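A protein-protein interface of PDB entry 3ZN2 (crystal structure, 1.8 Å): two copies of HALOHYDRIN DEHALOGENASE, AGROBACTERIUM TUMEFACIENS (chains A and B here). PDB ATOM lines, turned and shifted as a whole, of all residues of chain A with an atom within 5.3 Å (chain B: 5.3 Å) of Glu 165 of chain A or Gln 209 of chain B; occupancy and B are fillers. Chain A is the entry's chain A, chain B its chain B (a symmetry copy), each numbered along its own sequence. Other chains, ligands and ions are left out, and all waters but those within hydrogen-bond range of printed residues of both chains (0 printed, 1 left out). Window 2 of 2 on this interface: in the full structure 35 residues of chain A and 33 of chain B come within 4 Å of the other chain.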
ATOM      1  N   LYS A 123      30.358 -12.561 -13.918  1.00  0.00           N
ATOM      2  CA  LYS A 123      29.970 -12.069 -12.626  1.00  0.00           C
ATOM      3  C   LYS A 123      30.325 -10.618 -12.382  1.00  0.00           C
ATOM      4  O   LYS A 123      30.815 -10.262 -11.314  1.00  0.00           O
ATOM      5  CB  LYS A 123      30.497 -13.012 -11.522  1.00  0.00           C
ATOM      6  CG  LYS A 123      30.357 -14.482 -12.025  1.00  0.00           C
ATOM      7  CD  LYS A 123      30.013 -15.513 -10.973  1.00  0.00           C
ATOM      8  CE  LYS A 123      30.804 -15.313  -9.687  1.00  0.00           C
ATOM      9  NZ  LYS A 123      30.101 -14.414  -8.714  1.00  0.00           N
ATOM     10  N   LYS A 161      17.217  -9.103  -7.160  1.00  0.00           N
ATOM     11  CA  LYS A 161      17.193 -10.221  -6.255  1.00  0.00           C
ATOM     12  C   LYS A 161      17.861 -11.437  -6.948  1.00  0.00           C
ATOM     13  O   LYS A 161      18.539 -12.178  -6.309  1.00  0.00           O
ATOM     14  CB  LYS A 161      15.782 -10.602  -5.971  1.00  0.00           C
ATOM     15  CG  LYS A 161      14.982  -9.521  -5.299  1.00  0.00           C
ATOM     16  CD  LYS A 161      15.430  -9.139  -3.962  1.00  0.00           C
ATOM     17  CE  LYS A 161      14.397  -8.214  -3.308  1.00  0.00           C
ATOM     18  NZ  LYS A 161      14.965  -7.550  -2.111  1.00  0.00           N
ATOM     19  N   GLU A 162      17.696 -11.580  -8.230  1.00  0.00           N
ATOM     20  CA  GLU A 162      18.347 -12.709  -8.909  1.00  0.00           C
ATOM     21  C   GLU A 162      19.779 -12.455  -9.333  1.00  0.00           C
ATOM     22  O   GLU A 162      20.605 -13.407  -9.426  1.00  0.00           O
ATOM     23  CB  GLU A 162      17.550 -13.180 -10.096  1.00  0.00           C
ATOM     24  CG  GLU A 162      17.605 -12.382 -11.385  1.00  0.00           C
ATOM     25  CD  GLU A 162      16.609 -12.899 -12.393  1.00  0.00           C
ATOM     26  OE1 GLU A 162      15.410 -12.554 -12.233  1.00  0.00           O
ATOM     27  OE2 GLU A 162      17.028 -13.618 -13.364  1.00  0.00           O
ATOM     28  N   LEU A 163      20.079 -11.190  -9.621  1.00  0.00           N
ATOM     29  CA  LEU A 163      21.386 -10.827 -10.228  1.00  0.00           C
ATOM     30  C   LEU A 163      22.470 -10.573  -9.242  1.00  0.00           C
ATOM     31  O   LEU A 163      23.633 -10.602  -9.582  1.00  0.00           O
ATOM     32  CB  LEU A 163      21.198  -9.716 -11.286  1.00  0.00           C
ATOM     33  CG  LEU A 163      20.340 -10.091 -12.460  1.00  0.00           C
ATOM     34  CD1 LEU A 163      20.122  -8.988 -13.488  1.00  0.00           C
ATOM     35  CD2 LEU A 163      20.909 -11.285 -13.223  1.00  0.00           C
ATOM     36  N   GLY A 164      22.069 -10.382  -7.991  1.00  0.00           N
ATOM     37  CA  GLY A 164      22.910 -10.126  -6.849  1.00  0.00           C
ATOM     38  C   GLY A 164      23.912 -11.244  -6.677  1.00  0.00           C
ATOM     39  O   GLY A 164      25.060 -11.001  -6.276  1.00  0.00           O
ATOM     40  N   GLU A 165      23.435 -12.449  -6.989  1.00  0.00           N
ATOM     41  CA  GLU A 165      24.180 -13.691  -6.878  1.00  0.00           C
ATOM     42  C   GLU A 165      25.408 -13.630  -7.761  1.00  0.00           C
ATOM     43  O   GLU A 165      26.446 -14.190  -7.378  1.00  0.00           O
ATOM     44  CB  GLU A 165      23.286 -14.882  -7.328  1.00  0.00           C
ATOM     45  CG  GLU A 165      24.003 -16.214  -7.327  1.00  0.00           C
ATOM     46  CD  GLU A 165      23.095 -17.412  -7.606  1.00  0.00           C
ATOM     47  OE1 GLU A 165      21.877 -17.373  -7.263  1.00  0.00           O
ATOM     48  OE2 GLU A 165      23.641 -18.393  -8.178  1.00  0.00           O
ATOM     49  N   TYR A 166      25.261 -12.967  -8.946  1.00  0.00           N
ATOM     50  CA  TYR A 166      26.286 -12.759  -9.897  1.00  0.00           C
ATOM     51  C   TYR A 166      26.981 -11.373  -9.791  1.00  0.00           C
ATOM     52  O   TYR A 166      27.634 -10.978 -10.762  1.00  0.00           O
ATOM     53  CB  TYR A 166      25.700 -12.938 -11.284  1.00  0.00           C
ATOM     54  CG  TYR A 166      25.045 -14.245 -11.478  1.00  0.00           C
ATOM     55  CD1 TYR A 166      23.695 -14.424 -11.124  1.00  0.00           C
ATOM     56  CD2 TYR A 166      25.747 -15.346 -12.010  1.00  0.00           C
ATOM     57  CE1 TYR A 166      23.065 -15.622 -11.278  1.00  0.00           C
ATOM     58  CE2 TYR A 166      25.106 -16.586 -12.172  1.00  0.00           C
ATOM     59  CZ  TYR A 166      23.762 -16.700 -11.789  1.00  0.00           C
ATOM     60  OH  TYR A 166      23.075 -17.874 -11.893  1.00  0.00           O
ATOM     61  N   ASN A 167      26.890 -10.709  -8.631  1.00  0.00           N
ATOM     62  CA  ASN A 167      27.495  -9.387  -8.398  1.00  0.00           C
ATOM     63  C   ASN A 167      27.137  -8.402  -9.513  1.00  0.00           C
ATOM     64  O   ASN A 167      27.983  -7.694 -10.065  1.00  0.00           O
ATOM     65  CB  ASN A 167      29.023  -9.450  -8.240  1.00  0.00           C
ATOM     66  CG  ASN A 167      29.531  -8.486  -7.188  1.00  0.00           C
ATOM     67  OD1 ASN A 167      28.945  -8.387  -6.087  1.00  0.00           O
ATOM     68  ND2 ASN A 167      30.644  -7.796  -7.480  1.00  0.00           N
ATOM     69  N   VAL B 202      24.097 -14.141   6.339  1.00  0.00           N
ATOM     70  CA  VAL B 202      24.300 -12.962   5.449  1.00  0.00           C
ATOM     71  C   VAL B 202      24.210 -13.352   4.006  1.00  0.00           C
ATOM     72  O   VAL B 202      23.542 -12.676   3.199  1.00  0.00           O
ATOM     73  CB  VAL B 202      25.661 -12.314   5.724  1.00  0.00           C
ATOM     74  CG1 VAL B 202      26.168 -11.478   4.518  1.00  0.00           C
ATOM     75  CG2 VAL B 202      25.551 -11.511   6.986  1.00  0.00           C
ATOM     76  N   LYS B 203      24.835 -14.467   3.674  1.00  0.00           N
ATOM     77  CA  LYS B 203      24.793 -15.019   2.358  1.00  0.00           C
ATOM     78  C   LYS B 203      23.407 -15.374   1.846  1.00  0.00           C
ATOM     79  O   LYS B 203      23.105 -15.195   0.657  1.00  0.00           O
ATOM     80  CB  LYS B 203      25.723 -16.235   2.289  1.00  0.00           C
ATOM     81  CG  LYS B 203      26.213 -16.502   0.893  1.00  0.00           C
ATOM     82  CD  LYS B 203      26.744 -17.932   0.681  1.00  0.00           C
ATOM     83  CE  LYS B 203      26.108 -18.576  -0.559  1.00  0.00           C
ATOM     84  NZ  LYS B 203      27.079 -19.410  -1.313  1.00  0.00           N
ATOM     85  N   THR B 206      20.831 -11.541   1.949  1.00  0.00           N
ATOM     86  CA  THR B 206      21.201 -10.480   1.004  1.00  0.00           C
ATOM     87  C   THR B 206      21.313 -10.995  -0.389  1.00  0.00           C
ATOM     88  O   THR B 206      21.861 -12.114  -0.609  1.00  0.00           O
ATOM     89  CB  THR B 206      22.519  -9.749   1.408  1.00  0.00           C
ATOM     90  OG1 THR B 206      23.669 -10.629   1.333  1.00  0.00           O
ATOM     91  CG2 THR B 206      22.449  -9.132   2.793  1.00  0.00           C
ATOM     92  N   ALA B 207      20.832 -10.221  -1.389  1.00  0.00           N
ATOM     93  CA  ALA B 207      21.061 -10.607  -2.749  1.00  0.00           C
ATOM     94  C   ALA B 207      22.514 -10.633  -3.185  1.00  0.00           C
ATOM     95  O   ALA B 207      22.903 -11.435  -4.039  1.00  0.00           O
ATOM     96  CB  ALA B 207      20.254  -9.731  -3.708  1.00  0.00           C
ATOM     97  N   LEU B 208      23.305  -9.710  -2.689  1.00  0.00           N
ATOM     98  CA  LEU B 208      24.740  -9.674  -3.024  1.00  0.00           C
ATOM     99  C   LEU B 208      25.561 -10.617  -2.131  1.00  0.00           C
ATOM    100  O   LEU B 208      26.772 -10.774  -2.329  1.00  0.00           O
ATOM    101  CB  LEU B 208      25.250  -8.259  -2.889  1.00  0.00           C
ATOM    102  CG  LEU B 208      24.745  -7.347  -3.995  1.00  0.00           C
ATOM    103  CD1 LEU B 208      25.106  -5.907  -3.637  1.00  0.00           C
ATOM    104  CD2 LEU B 208      25.308  -7.715  -5.365  1.00  0.00           C
ATOM    105  N   GLN B 209      24.925 -11.168  -1.105  1.00  0.00           N
ATOM    106  CA  GLN B 209      25.463 -12.305  -0.373  1.00  0.00           C
ATOM    107  C   GLN B 209      26.712 -11.876   0.315  1.00  0.00           C
ATOM    108  O   GLN B 209      27.686 -12.578   0.268  1.00  0.00           O
ATOM    109  CB  GLN B 209      25.724 -13.549  -1.308  1.00  0.00           C
ATOM    110  CG  GLN B 209      24.571 -13.934  -2.190  1.00  0.00           C
ATOM    111  CD  GLN B 209      24.702 -15.297  -2.844  1.00  0.00           C
ATOM    112  OE1 GLN B 209      25.471 -15.490  -3.758  1.00  0.00           O
ATOM    113  NE2 GLN B 209      23.865 -16.214  -2.432  1.00  0.00           N
ATOM    114  N   ARG B 210      26.667 -10.749   1.017  1.00  0.00           N
ATOM    115  CA  ARG B 210      27.784 -10.214   1.731  1.00  0.00           C
ATOM    116  C   ARG B 210      27.301  -9.083   2.563  1.00  0.00           C
ATOM    117  O   ARG B 210      26.235  -8.547   2.305  1.00  0.00           O
ATOM    118  CB  ARG B 210      28.872  -9.718   0.797  1.00  0.00           C
ATOM    119  CG  ARG B 210      28.389  -8.698  -0.281  1.00  0.00           C
ATOM    120  CD  ARG B 210      29.589  -7.925  -0.697  1.00  0.00           C
ATOM    121  NE  ARG B 210      29.282  -6.956  -1.692  1.00  0.00           N
ATOM    122  CZ  ARG B 210      29.138  -5.654  -1.483  1.00  0.00           C
ATOM    123  NH1 ARG B 210      29.215  -5.166  -0.290  1.00  0.00           N
ATOM    124  NH2 ARG B 210      28.898  -4.869  -2.502  1.00  0.00           N
ATOM    125  N   LEU B 211      28.102  -8.716   3.539  1.00  0.00           N
ATOM    126  CA  LEU B 211      27.964  -7.446   4.241  1.00  0.00           C
ATOM    127  C   LEU B 211      28.259  -6.250   3.364  1.00  0.00           C
ATOM    128  O   LEU B 211      29.004  -6.340   2.379  1.00  0.00           O
ATOM    129  CB  LEU B 211      28.901  -7.389   5.421  1.00  0.00           C
ATOM    130  CG  LEU B 211      28.782  -8.518   6.457  1.00  0.00           C
ATOM    131  CD1 LEU B 211      29.914  -8.311   7.494  1.00  0.00           C
ATOM    132  CD2 LEU B 211      27.414  -8.533   7.169  1.00  0.00           C
ATOM    133  N   GLY B 241      21.973  -4.241   0.297  1.00  0.00           N
ATOM    134  CA  GLY B 241      22.390  -5.331  -0.549  1.00  0.00           C
ATOM    135  C   GLY B 241      21.329  -6.219  -1.089  1.00  0.00           C
ATOM    136  O   GLY B 241      21.573  -7.381  -1.429  1.00  0.00           O
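Printed residues of chain B within 4 Å of Lys 161 of chain A: Ala 207. Of the printed residues of chain B, Gly 164 of chain A touches Ala 207 (2.8 Å) and Leu 208 (3.4 Å). Glu 165 of chain A touches just these residues of chain B: Ala 207 and Gln 209. Tyr 166 of chain A touches none of the printed residues of chain B. Of the printed residues of chain B, Asn 167 of chain A touches Leu 208 (3.8 Å). Printed residues of chain A within 4 Å of Ala 207 of chain B: Lys 161, Gly 164 and Glu 165. Printed residues of chain A within 4 Å of Leu 208 of chain B: Gly 164 and Asn 167. Of chain A, only Glu 165 (3.8 Å) comes within 4 Å of Gln 209 of chain B. The nearest residue of chain B that does not touch Glu 165 of chain A is Leu 208 of chain B (5.0 Å). The nearest residue of chain A that does not touch Gln 209 of chain B is Gly 164 of chain A (5.1 Å). The nearest printed residue of chain B that does not touch Asn 167 of chain A is Arg 210 of chain B (4.6 Å).
O of Lys 161 of chain A touches CB of Ala 207 of chain B (3.96 Å). O of Gly 164 of chain A touches CD2 of Leu 208 of chain B, at 3.4 Å. Glu 165 of chain A touches Gln 209 of chain B. Asn 167 of chain A touches Leu 208 of chain B.
The backbone NH (N) of Glu 165 of chain A lies within hydrogen-bond range of the backbone carbonyl oxygen (O) of Ala 207 of chain B, at 3.2 Å. O of Ala 207 of chain B lies close to O of Gly 164 of chain A.
No position is printed for both chains.
O of Lys 203 of chain B is in hydrogen-bond range of NE2 of Gln 209 of chain B. The side-chain hydroxyl (OG1) of Thr 206 of chain B is in hydrogen-bond range of the backbone NH (N) of Gln 209 of chain B (2.8 Å). The backbone NH (N) of Ala 207 of chain B sits at hydrogen-bond distance from the backbone carbonyl oxygen (O) of Gly 241 of chain B, at 2.9 Å. The backbone NH (N) of Leu 208 of chain B lies within hydrogen-bond range of the backbone carbonyl oxygen (O) of Gly 241 of chain B (3.2 Å).
Of the 8 printed residues of chain A, 4 touch a printed residue of chain B. Of the 9 printed residues of chain B, 3 touch a printed residue of chain A. Along chain B the printed residues that touch a printed residue of chain A span positions 207 to 209. Among the printed residues, no Asp or Glu carboxylate lies within 4 Å of a Lys or Arg side-chain nitrogen of the other chain.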
